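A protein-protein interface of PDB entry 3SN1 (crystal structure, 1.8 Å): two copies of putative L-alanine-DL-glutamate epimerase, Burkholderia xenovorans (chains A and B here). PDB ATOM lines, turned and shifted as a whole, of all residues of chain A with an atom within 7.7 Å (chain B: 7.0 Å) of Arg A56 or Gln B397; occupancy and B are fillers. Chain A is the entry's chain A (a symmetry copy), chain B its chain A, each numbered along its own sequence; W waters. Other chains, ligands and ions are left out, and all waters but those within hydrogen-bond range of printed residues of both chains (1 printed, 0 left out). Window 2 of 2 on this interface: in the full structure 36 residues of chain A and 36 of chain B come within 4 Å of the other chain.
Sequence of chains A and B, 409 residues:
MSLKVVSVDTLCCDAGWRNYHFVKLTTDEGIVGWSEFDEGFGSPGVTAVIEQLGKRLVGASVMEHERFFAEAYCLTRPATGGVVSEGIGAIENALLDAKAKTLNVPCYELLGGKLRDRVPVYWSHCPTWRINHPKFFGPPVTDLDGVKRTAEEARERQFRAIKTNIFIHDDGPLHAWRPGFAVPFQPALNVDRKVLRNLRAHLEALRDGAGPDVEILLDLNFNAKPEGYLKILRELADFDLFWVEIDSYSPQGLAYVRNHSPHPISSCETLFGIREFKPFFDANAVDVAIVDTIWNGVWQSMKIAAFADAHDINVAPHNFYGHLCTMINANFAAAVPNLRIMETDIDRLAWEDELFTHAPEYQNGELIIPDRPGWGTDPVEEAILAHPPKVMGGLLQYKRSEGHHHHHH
NH1 of Arg A56 is in hydrogen-bond range of O of Gln B397.
O of Gly B40 sits at hydrogen-bond distance from N of Leu B395 (2.9 Å).
NH2 of Arg A56 is in salt-bridge range of OE2 of Glu A71 (3.0 Å).
Among the printed residues, merely in contact across the chains: Gln A52 with Met B392 (3.2 Å), Leu A75 with Phe B181 (3.7 Å) and Leu A75 with Leu B395 (3.4 Å).
Of chain B, only Gln B397 comes within 4 Å of Arg A56.
Gln B397 touches just one residue of chain A: Arg A56.
Printed residues of chain A within 4 Å of Leu B395: Leu A75 (3.4 Å).
Of the printed residues of chain B, Leu A75 touches Phe B181 and Leu B395.
Of the printed residues of chain A, Met B392 touches Gln A52 (3.2 Å).
Ile A50 touches none of the printed residues of chain B.
Val A8 touches none of the printed residues of chain B.
The nearest printed residue of chain A that does not touch Gln B397 is Leu A75 (6.2 Å).
Of the 17 printed residues of chain B, 4 touch a printed residue of chain A.
Printed residues of chain B that touch a printed residue of chain A: Phe B181, Met B392, Leu B395 and Gln B397.
Printed residues of chain A that touch a printed residue of chain B: Gln A52, Arg A56 and Leu A75.
Among the printed residues, no Asp or Glu carboxylate lies within 4 Å of a Lys or Arg side-chain nitrogen of the other chain.
No position is printed for both chains.
Of the 4 pairs that touch across the chains among the printed residues, none has its exchanged pair printed and touching as well.
Water W1 lies within hydrogen-bond range of N of Met B392 (2.9 Å) and NE2 of Gln A52 (3.2 Å).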
ATOM      1  N   VAL A   5     -26.772  11.966  41.317  1.00  0.00           N
ATOM      2  CA  VAL A   5     -27.626  10.837  40.978  1.00  0.00           C
ATOM      3  C   VAL A   5     -27.090   9.631  41.741  1.00  0.00           C
ATOM      4  O   VAL A   5     -25.882   9.351  41.692  1.00  0.00           O
ATOM      5  CB  VAL A   5     -27.618  10.557  39.465  1.00  0.00           C
ATOM      6  CG1 VAL A   5     -28.346   9.248  39.145  1.00  0.00           C
ATOM      7  CG2 VAL A   5     -28.244  11.742  38.679  1.00  0.00           C
ATOM      8  N   VAL A   8     -30.082   4.659  38.780  1.00  0.00           N
ATOM      9  CA  VAL A   8     -30.886   4.706  37.589  1.00  0.00           C
ATOM     10  C   VAL A   8     -31.384   3.283  37.402  1.00  0.00           C
ATOM     11  O   VAL A   8     -30.584   2.365  37.238  1.00  0.00           O
ATOM     12  CB  VAL A   8     -30.066   5.120  36.354  1.00  0.00           C
ATOM     13  CG1 VAL A   8     -30.933   5.126  35.105  1.00  0.00           C
ATOM     14  CG2 VAL A   8     -29.387   6.475  36.587  1.00  0.00           C
ATOM     15  N   ILE A  50     -30.222   2.006  28.169  1.00  0.00           N
ATOM     16  CA  ILE A  50     -30.414   2.728  29.422  1.00  0.00           C
ATOM     17  C   ILE A  50     -29.579   2.153  30.560  1.00  0.00           C
ATOM     18  O   ILE A  50     -28.956   2.896  31.321  1.00  0.00           O
ATOM     19  CB  ILE A  50     -31.909   2.735  29.820  1.00  0.00           C
ATOM     20  CG1 ILE A  50     -32.678   3.571  28.815  1.00  0.00           C
ATOM     21  CG2 ILE A  50     -32.071   3.309  31.227  1.00  0.00           C
ATOM     22  CD1 ILE A  50     -34.206   3.420  28.869  1.00  0.00           C
ATOM     23  N   GLU A  51     -29.556   0.837  30.678  1.00  0.00           N
ATOM     24  CA  GLU A  51     -28.819   0.228  31.778  1.00  0.00           C
ATOM     25  C   GLU A  51     -27.308   0.486  31.662  1.00  0.00           C
ATOM     26  O   GLU A  51     -26.654   0.700  32.681  1.00  0.00           O
ATOM     27  CB  GLU A  51     -29.168  -1.256  31.918  1.00  0.00           C
ATOM     28  CG  GLU A  51     -30.645  -1.486  32.350  1.00  0.00           C
ATOM     29  CD  GLU A  51     -30.884  -1.304  33.852  1.00  0.00           C
ATOM     30  OE1 GLU A  51     -32.055  -1.364  34.287  1.00  0.00           O
ATOM     31  OE2 GLU A  51     -29.903  -1.105  34.596  1.00  0.00           O
ATOM     32  N   GLN A  52     -26.772   0.515  30.439  1.00  0.00           N
ATOM     33  CA  GLN A  52     -25.357   0.842  30.228  1.00  0.00           C
ATOM     34  C   GLN A  52     -25.098   2.312  30.510  1.00  0.00           C
ATOM     35  O   GLN A  52     -24.184   2.649  31.248  1.00  0.00           O
ATOM     36  CB  GLN A  52     -24.912   0.535  28.798  1.00  0.00           C
ATOM     37  CG  GLN A  52     -24.735  -0.927  28.501  1.00  0.00           C
ATOM     38  CD  GLN A  52     -23.927  -1.664  29.560  1.00  0.00           C
ATOM     39  OE1 GLN A  52     -22.931  -1.155  30.082  1.00  0.00           O
ATOM     40  NE2 GLN A  52     -24.361  -2.875  29.888  1.00  0.00           N
ATOM     41  N   LEU A  53     -25.899   3.197  29.906  1.00  0.00           N
ATOM     42  CA  LEU A  53     -25.671   4.628  30.069  1.00  0.00           C
ATOM     43  C   LEU A  53     -25.892   5.139  31.487  1.00  0.00           C
ATOM     44  O   LEU A  53     -25.199   6.060  31.939  1.00  0.00           O
ATOM     45  CB  LEU A  53     -26.516   5.421  29.083  1.00  0.00           C
ATOM     46  CG  LEU A  53     -26.120   5.274  27.615  1.00  0.00           C
ATOM     47  CD1 LEU A  53     -27.117   6.077  26.771  1.00  0.00           C
ATOM     48  CD2 LEU A  53     -24.676   5.767  27.373  1.00  0.00           C
ATOM     49  N   GLY A  54     -26.855   4.546  32.193  1.00  0.00           N
ATOM     50  CA  GLY A  54     -27.112   4.912  33.578  1.00  0.00           C
ATOM     51  C   GLY A  54     -25.966   4.619  34.521  1.00  0.00           C
ATOM     52  O   GLY A  54     -25.787   5.317  35.521  1.00  0.00           O
ATOM     53  N   LYS A  55     -25.173   3.599  34.213  1.00  0.00           N
ATOM     54  CA  LYS A  55     -23.958   3.338  34.981  1.00  0.00           C
ATOM     55  C   LYS A  55     -23.014   4.541  35.029  1.00  0.00           C
ATOM     56  O   LYS A  55     -22.409   4.795  36.064  1.00  0.00           O
ATOM     57  CB  LYS A  55     -23.221   2.113  34.431  1.00  0.00           C
ATOM     58  CG  LYS A  55     -24.003   0.823  34.681  1.00  0.00           C
ATOM     59  CD  LYS A  55     -23.305  -0.422  34.175  1.00  0.00           C
ATOM     60  CE  LYS A  55     -24.283  -1.604  34.180  1.00  0.00           C
ATOM     61  NZ  LYS A  55     -23.640  -2.884  34.621  1.00  0.00           N
ATOM     62  N   ARG A  56     -22.885   5.261  33.918  1.00  0.00           N
ATOM     63  CA  ARG A  56     -21.971   6.408  33.830  1.00  0.00           C
ATOM     64  C   ARG A  56     -22.559   7.603  34.549  1.00  0.00           C
ATOM     65  O   ARG A  56     -21.837   8.460  35.056  1.00  0.00           O
ATOM     66  CB  ARG A  56     -21.727   6.831  32.379  1.00  0.00           C
ATOM     67  CG  ARG A  56     -21.148   5.765  31.457  1.00  0.00           C
ATOM     68  CD  ARG A  56     -19.619   5.696  31.544  1.00  0.00           C
ATOM     69  NE  ARG A  56     -18.952   6.963  31.193  1.00  0.00           N
ATOM     70  CZ  ARG A  56     -17.862   7.059  30.420  1.00  0.00           C
ATOM     71  NH1 ARG A  56     -17.307   5.976  29.872  1.00  0.00           N
ATOM     72  NH2 ARG A  56     -17.327   8.256  30.166  1.00  0.00           N
ATOM     73  N   LEU A  57     -23.878   7.652  34.597  1.00  0.00           N
ATOM     74  CA  LEU A  57     -24.567   8.782  35.194  1.00  0.00           C
ATOM     75  C   LEU A  57     -24.490   8.786  36.719  1.00  0.00           C
ATOM     76  O   LEU A  57     -24.439   9.864  37.323  1.00  0.00           O
ATOM     77  CB  LEU A  57     -26.022   8.824  34.697  1.00  0.00           C
ATOM     78  CG  LEU A  57     -26.908   9.978  35.168  1.00  0.00           C
ATOM     79  CD1 LEU A  57     -26.344  11.372  34.766  1.00  0.00           C
ATOM     80  CD2 LEU A  57     -28.335   9.787  34.643  1.00  0.00           C
ATOM     81  N   VAL A  58     -24.457   7.613  37.370  1.00  0.00           N
ATOM     82  CA  VAL A  58     -24.368   7.588  38.832  1.00  0.00           C
ATOM     83  C   VAL A  58     -23.117   8.329  39.331  1.00  0.00           C
ATOM     84  O   VAL A  58     -22.005   8.104  38.840  1.00  0.00           O
ATOM     85  CB  VAL A  58     -24.373   6.136  39.385  1.00  0.00           C
ATOM     86  CG1 VAL A  58     -24.054   6.104  40.865  1.00  0.00           C
ATOM     87  CG2 VAL A  58     -25.750   5.471  39.102  1.00  0.00           C
ATOM     88  N   GLY A  59     -23.316   9.227  40.294  1.00  0.00           N
ATOM     89  CA  GLY A  59     -22.257  10.075  40.813  1.00  0.00           C
ATOM     90  C   GLY A  59     -22.185  11.453  40.168  1.00  0.00           C
ATOM     91  O   GLY A  59     -21.533  12.348  40.711  1.00  0.00           O
ATOM     92  N   ALA A  60     -22.847  11.624  39.025  1.00  0.00           N
ATOM     93  CA  ALA A  60     -22.906  12.915  38.335  1.00  0.00           C
ATOM     94  C   ALA A  60     -24.029  13.773  38.915  1.00  0.00           C
ATOM     95  O   ALA A  60     -24.883  13.280  39.656  1.00  0.00           O
ATOM     96  CB  ALA A  60     -23.108  12.723  36.835  1.00  0.00           C
ATOM     97  N   ARG A  67     -24.996  18.134  29.933  1.00  0.00           N
ATOM     98  CA  ARG A  67     -23.695  17.474  30.082  1.00  0.00           C
ATOM     99  C   ARG A  67     -23.838  15.969  29.857  1.00  0.00           C
ATOM    100  O   ARG A  67     -23.066  15.365  29.094  1.00  0.00           O
ATOM    101  CB  ARG A  67     -23.111  17.737  31.469  1.00  0.00           C
ATOM    102  CG  ARG A  67     -21.672  17.238  31.648  1.00  0.00           C
ATOM    103  CD  ARG A  67     -21.378  16.760  33.093  1.00  0.00           C
ATOM    104  NE  ARG A  67     -22.250  15.666  33.506  1.00  0.00           N
ATOM    105  CZ  ARG A  67     -22.134  14.393  33.121  1.00  0.00           C
ATOM    106  NH1 ARG A  67     -21.135  13.995  32.331  1.00  0.00           N
ATOM    107  NH2 ARG A  67     -23.023  13.509  33.533  1.00  0.00           N
ATOM    108  N   PHE A  68     -24.807  15.349  30.533  1.00  0.00           N
ATOM    109  CA  PHE A  68     -25.052  13.918  30.340  1.00  0.00           C
ATOM    110  C   PHE A  68     -25.351  13.616  28.870  1.00  0.00           C
ATOM    111  O   PHE A  68     -24.825  12.648  28.310  1.00  0.00           O
ATOM    112  CB  PHE A  68     -26.219  13.399  31.197  1.00  0.00           C
ATOM    113  CG  PHE A  68     -26.787  12.097  30.677  1.00  0.00           C
ATOM    114  CD1 PHE A  68     -26.147  10.916  30.944  1.00  0.00           C
ATOM    115  CD2 PHE A  68     -27.913  12.088  29.863  1.00  0.00           C
ATOM    116  CE1 PHE A  68     -26.610   9.716  30.434  1.00  0.00           C
ATOM    117  CE2 PHE A  68     -28.402  10.878  29.320  1.00  0.00           C
ATOM    118  CZ  PHE A  68     -27.736   9.694  29.623  1.00  0.00           C
ATOM    119  N   GLU A  71     -22.221  13.836  26.750  1.00  0.00           N
ATOM    120  CA  GLU A  71     -21.346  12.710  27.016  1.00  0.00           C
ATOM    121  C   GLU A  71     -21.899  11.438  26.365  1.00  0.00           C
ATOM    122  O   GLU A  71     -21.171  10.669  25.738  1.00  0.00           O
ATOM    123  CB  GLU A  71     -21.178  12.490  28.517  1.00  0.00           C
ATOM    124  CG  GLU A  71     -20.235  11.345  28.847  1.00  0.00           C
ATOM    125  CD  GLU A  71     -20.003  11.147  30.332  1.00  0.00           C
ATOM    126  OE1 GLU A  71     -20.923  11.361  31.128  1.00  0.00           O
ATOM    127  OE2 GLU A  71     -18.893  10.738  30.711  1.00  0.00           O
ATOM    128  N   ALA A  72     -23.194  11.209  26.545  1.00  0.00           N
ATOM    129  CA  ALA A  72     -23.838  10.013  26.009  1.00  0.00           C
ATOM    130  C   ALA A  72     -23.771   9.957  24.498  1.00  0.00           C
ATOM    131  O   ALA A  72     -23.549   8.898  23.909  1.00  0.00           O
ATOM    132  CB  ALA A  72     -25.305   9.953  26.481  1.00  0.00           C
ATOM    133  N   LEU A  75     -20.308   8.793  23.585  1.00  0.00           N
ATOM    134  CA  LEU A  75     -20.041   7.390  23.873  1.00  0.00           C
ATOM    135  C   LEU A  75     -20.752   6.420  22.909  1.00  0.00           C
ATOM    136  O   LEU A  75     -20.303   5.273  22.751  1.00  0.00           O
ATOM    137  CB  LEU A  75     -20.478   7.067  25.298  1.00  0.00           C
ATOM    138  CG  LEU A  75     -19.751   7.793  26.418  1.00  0.00           C
ATOM    139  CD1 LEU A  75     -20.396   7.447  27.785  1.00  0.00           C
ATOM    140  CD2 LEU A  75     -18.282   7.442  26.394  1.00  0.00           C
ATOM    141  N   GLY B  16     -10.524  -8.759  25.812  1.00  0.00           N
ATOM    142  CA  GLY B  16      -9.547  -7.991  26.585  1.00  0.00           C
ATOM    143  C   GLY B  16     -10.143  -6.705  27.132  1.00  0.00           C
ATOM    144  O   GLY B  16     -10.429  -6.609  28.323  1.00  0.00           O
ATOM    145  N   TRP B  17     -10.292  -5.733  26.244  1.00  0.00           N
ATOM    146  CA  TRP B  17     -10.818  -4.397  26.557  1.00  0.00           C
ATOM    147  C   TRP B  17     -12.211  -4.210  25.975  1.00  0.00           C
ATOM    148  O   TRP B  17     -12.804  -3.128  26.048  1.00  0.00           O
ATOM    149  CB  TRP B  17      -9.872  -3.325  25.987  1.00  0.00           C
ATOM    150  CG  TRP B  17      -9.628  -3.448  24.543  1.00  0.00           C
ATOM    151  CD1 TRP B  17      -8.786  -4.336  23.924  1.00  0.00           C
ATOM    152  CD2 TRP B  17     -10.224  -2.677  23.503  1.00  0.00           C
ATOM    153  NE1 TRP B  17      -8.823  -4.156  22.575  1.00  0.00           N
ATOM    154  CE2 TRP B  17      -9.697  -3.147  22.281  1.00  0.00           C
ATOM    155  CE3 TRP B  17     -11.154  -1.632  23.481  1.00  0.00           C
ATOM    156  CZ2 TRP B  17     -10.064  -2.607  21.056  1.00  0.00           C
ATOM    157  CZ3 TRP B  17     -11.508  -1.080  22.255  1.00  0.00           C
ATOM    158  CH2 TRP B  17     -10.975  -1.580  21.061  1.00  0.00           C
ATOM    159  N   ARG B  18     -12.699  -5.274  25.347  1.00  0.00           N
ATOM    160  CA  ARG B  18     -14.024  -5.358  24.759  1.00  0.00           C
ATOM    161  C   ARG B  18     -14.375  -6.850  24.664  1.00  0.00           C
ATOM    162  O   ARG B  18     -13.525  -7.713  24.893  1.00  0.00           O
ATOM    163  CB  ARG B  18     -14.041  -4.726  23.369  1.00  0.00           C
ATOM    164  CG  ARG B  18     -13.084  -5.412  22.403  1.00  0.00           C
ATOM    165  CD  ARG B  18     -13.041  -4.717  21.092  1.00  0.00           C
ATOM    166  NE  ARG B  18     -12.023  -5.324  20.238  1.00  0.00           N
ATOM    167  CZ  ARG B  18     -11.816  -5.019  18.964  1.00  0.00           C
ATOM    168  NH1 ARG B  18     -12.583  -4.114  18.349  1.00  0.00           N
ATOM    169  NH2 ARG B  18     -10.849  -5.656  18.290  1.00  0.00           N
ATOM    170  N   GLY B  40     -19.373  -2.968  21.621  1.00  0.00           N
ATOM    171  CA  GLY B  40     -18.487  -2.011  22.295  1.00  0.00           C
ATOM    172  C   GLY B  40     -18.331  -0.704  21.549  1.00  0.00           C
ATOM    173  O   GLY B  40     -18.090   0.333  22.163  1.00  0.00           O
ATOM    174  N   HIS B 133      -3.949  -0.167  24.055  1.00  0.00           N
ATOM    175  CA  HIS B 133      -4.275  -1.382  24.786  1.00  0.00           C
ATOM    176  C   HIS B 133      -3.040  -2.275  24.980  1.00  0.00           C
ATOM    177  O   HIS B 133      -3.048  -3.445  24.586  1.00  0.00           O
ATOM    178  CB  HIS B 133      -5.406  -2.112  24.055  1.00  0.00           C
ATOM    179  CG  HIS B 133      -6.582  -1.241  23.754  1.00  0.00           C
ATOM    180  ND1 HIS B 133      -7.426  -0.769  24.737  1.00  0.00           N
ATOM    181  CD2 HIS B 133      -7.020  -0.704  22.593  1.00  0.00           C
ATOM    182  CE1 HIS B 133      -8.345   0.005  24.188  1.00  0.00           C
ATOM    183  NE2 HIS B 133      -8.131   0.055  22.889  1.00  0.00           N
ATOM    184  N   PHE B 136      -2.816  -5.916  26.165  1.00  0.00           N
ATOM    185  CA  PHE B 136      -3.303  -6.951  25.237  1.00  0.00           C
ATOM    186  C   PHE B 136      -2.516  -7.109  23.958  1.00  0.00           C
ATOM    187  O   PHE B 136      -2.442  -8.225  23.400  1.00  0.00           O
ATOM    188  CB  PHE B 136      -4.786  -6.699  24.947  1.00  0.00           C
ATOM    189  CG  PHE B 136      -5.602  -6.707  26.184  1.00  0.00           C
ATOM    190  CD1 PHE B 136      -5.769  -7.895  26.901  1.00  0.00           C
ATOM    191  CD2 PHE B 136      -6.114  -5.534  26.706  1.00  0.00           C
ATOM    192  CE1 PHE B 136      -6.480  -7.918  28.076  1.00  0.00           C
ATOM    193  CE2 PHE B 136      -6.820  -5.552  27.897  1.00  0.00           C
ATOM    194  CZ  PHE B 136      -7.008  -6.741  28.576  1.00  0.00           C
ATOM    195  N   PHE B 181     -15.292  10.696  21.204  1.00  0.00           N
ATOM    196  CA  PHE B 181     -15.806   9.594  22.034  1.00  0.00           C
ATOM    197  C   PHE B 181     -15.626   9.876  23.526  1.00  0.00           C
ATOM    198  O   PHE B 181     -15.609   8.946  24.370  1.00  0.00           O
ATOM    199  CB  PHE B 181     -15.122   8.274  21.631  1.00  0.00           C
ATOM    200  CG  PHE B 181     -15.300   7.876  20.182  1.00  0.00           C
ATOM    201  CD1 PHE B 181     -16.474   8.151  19.469  1.00  0.00           C
ATOM    202  CD2 PHE B 181     -14.293   7.155  19.532  1.00  0.00           C
ATOM    203  CE1 PHE B 181     -16.620   7.755  18.151  1.00  0.00           C
ATOM    204  CE2 PHE B 181     -14.431   6.754  18.216  1.00  0.00           C
ATOM    205  CZ  PHE B 181     -15.598   7.062  17.506  1.00  0.00           C
ATOM    206  N   ALA B 182     -15.529  11.166  23.861  1.00  0.00           N
ATOM    207  CA  ALA B 182     -15.485  11.643  25.230  1.00  0.00           C
ATOM    208  C   ALA B 182     -14.216  11.253  26.020  1.00  0.00           C
ATOM    209  O   ALA B 182     -14.234  11.243  27.257  1.00  0.00           O
ATOM    210  CB  ALA B 182     -16.752  11.216  25.978  1.00  0.00           C
ATOM    211  N   VAL B 183     -13.120  10.964  25.314  1.00  0.00           N
ATOM    212  CA  VAL B 183     -11.807  10.792  25.947  1.00  0.00           C
ATOM    213  C   VAL B 183     -10.774  11.720  25.284  1.00  0.00           C
ATOM    214  O   VAL B 183     -10.174  11.359  24.282  1.00  0.00           O
ATOM    215  CB  VAL B 183     -11.320   9.336  25.879  1.00  0.00           C
ATOM    216  CG1 VAL B 183      -9.971   9.197  26.621  1.00  0.00           C
ATOM    217  CG2 VAL B 183     -12.367   8.408  26.502  1.00  0.00           C
ATOM    218  N   LYS B 390     -16.399  -9.913  29.946  1.00  0.00           N
ATOM    219  CA  LYS B 390     -16.461  -8.919  31.025  1.00  0.00           C
ATOM    220  C   LYS B 390     -17.653  -8.043  30.750  1.00  0.00           C
ATOM    221  O   LYS B 390     -18.393  -8.263  29.789  1.00  0.00           O
ATOM    222  CB  LYS B 390     -15.186  -8.072  31.076  1.00  0.00           C
ATOM    223  CG  LYS B 390     -13.902  -8.866  31.285  1.00  0.00           C
ATOM    224  CD  LYS B 390     -12.647  -8.025  30.964  1.00  0.00           C
ATOM    225  CE  LYS B 390     -11.351  -8.813  31.195  1.00  0.00           C
ATOM    226  NZ  LYS B 390     -10.179  -8.122  30.527  1.00  0.00           N
ATOM    227  N   VAL B 391     -17.857  -7.030  31.583  1.00  0.00           N
ATOM    228  CA  VAL B 391     -18.899  -6.081  31.279  1.00  0.00           C
ATOM    229  C   VAL B 391     -18.486  -5.378  29.990  1.00  0.00           C
ATOM    230  O   VAL B 391     -17.339  -5.503  29.546  1.00  0.00           O
ATOM    231  CB  VAL B 391     -19.132  -5.082  32.423  1.00  0.00           C
ATOM    232  CG1 VAL B 391     -19.677  -5.834  33.681  1.00  0.00           C
ATOM    233  CG2 VAL B 391     -17.848  -4.300  32.693  1.00  0.00           C
ATOM    234  N   MET B 392     -19.416  -4.650  29.393  1.00  0.00           N
ATOM    235  CA  MET B 392     -19.143  -3.947  28.156  1.00  0.00           C
ATOM    236  C   MET B 392     -17.924  -3.036  28.275  1.00  0.00           C
ATOM    237  O   MET B 392     -17.793  -2.292  29.251  1.00  0.00           O
ATOM    238  CB  MET B 392     -20.361  -3.121  27.738  1.00  0.00           C
ATOM    239  CG  MET B 392     -20.315  -2.704  26.293  1.00  0.00           C
ATOM    240  SD  MET B 392     -21.983  -1.760  25.847  1.00  0.00           S
ATOM    241  CE  MET B 392     -23.249  -3.080  26.575  1.00  0.00           C
ATOM    242  N   GLY B 393     -17.046  -3.109  27.271  1.00  0.00           N
ATOM    243  CA  GLY B 393     -15.869  -2.250  27.161  1.00  0.00           C
ATOM    244  C   GLY B 393     -16.013  -1.371  25.924  1.00  0.00           C
ATOM    245  O   GLY B 393     -17.051  -0.740  25.730  1.00  0.00           O
ATOM    246  N   GLY B 394     -14.992  -1.345  25.078  1.00  0.00           N
ATOM    247  CA  GLY B 394     -15.021  -0.512  23.879  1.00  0.00           C
ATOM    248  C   GLY B 394     -15.147   0.945  24.278  1.00  0.00           C
ATOM    249  O   GLY B 394     -14.499   1.388  25.228  1.00  0.00           O
ATOM    250  N   LEU B 395     -16.005   1.691  23.585  1.00  0.00           N
ATOM    251  CA  LEU B 395     -16.226   3.101  23.919  1.00  0.00           C
ATOM    252  C   LEU B 395     -16.889   3.296  25.266  1.00  0.00           C
ATOM    253  O   LEU B 395     -16.813   4.385  25.829  1.00  0.00           O
ATOM    254  CB  LEU B 395     -17.104   3.795  22.872  1.00  0.00           C
ATOM    255  CG  LEU B 395     -16.655   3.746  21.422  1.00  0.00           C
ATOM    256  CD1 LEU B 395     -17.586   4.651  20.588  1.00  0.00           C
ATOM    257  CD2 LEU B 395     -15.205   4.152  21.246  1.00  0.00           C
ATOM    258  N   LEU B 396     -17.555   2.254  25.767  1.00  0.00           N
ATOM    259  CA  LEU B 396     -18.343   2.355  26.989  1.00  0.00           C
ATOM    260  C   LEU B 396     -17.567   1.877  28.203  1.00  0.00           C
ATOM    261  O   LEU B 396     -18.166   1.635  29.245  1.00  0.00           O
ATOM    262  CB  LEU B 396     -19.661   1.578  26.838  1.00  0.00           C
ATOM    263  CG  LEU B 396     -20.605   2.269  25.843  1.00  0.00           C
ATOM    264  CD1 LEU B 396     -20.943   1.362  24.654  1.00  0.00           C
ATOM    265  CD2 LEU B 396     -21.855   2.812  26.542  1.00  0.00           C
ATOM    266  N   GLN B 397     -16.241   1.761  28.067  1.00  0.00           N
ATOM    267  CA  GLN B 397     -15.347   1.466  29.187  1.00  0.00           C
ATOM    268  C   GLN B 397     -15.229   2.710  30.068  1.00  0.00           C
ATOM    269  O   GLN B 397     -16.238   3.261  30.515  1.00  0.00           O
ATOM    270  CB  GLN B 397     -13.953   1.048  28.672  1.00  0.00           C
ATOM    271  CG  GLN B 397     -13.060   0.333  29.707  1.00  0.00           C
ATOM    272  CD  GLN B 397     -12.132  -0.734  29.076  1.00  0.00           C
ATOM    273  OE1 GLN B 397     -11.520  -0.511  28.028  1.00  0.00           O
ATOM    274  NE2 GLN B 397     -12.031  -1.894  29.729  1.00  0.00           N
HETATM  275  O   HOH W   1     -22.053  -4.939  30.530  1.00  0.00           O
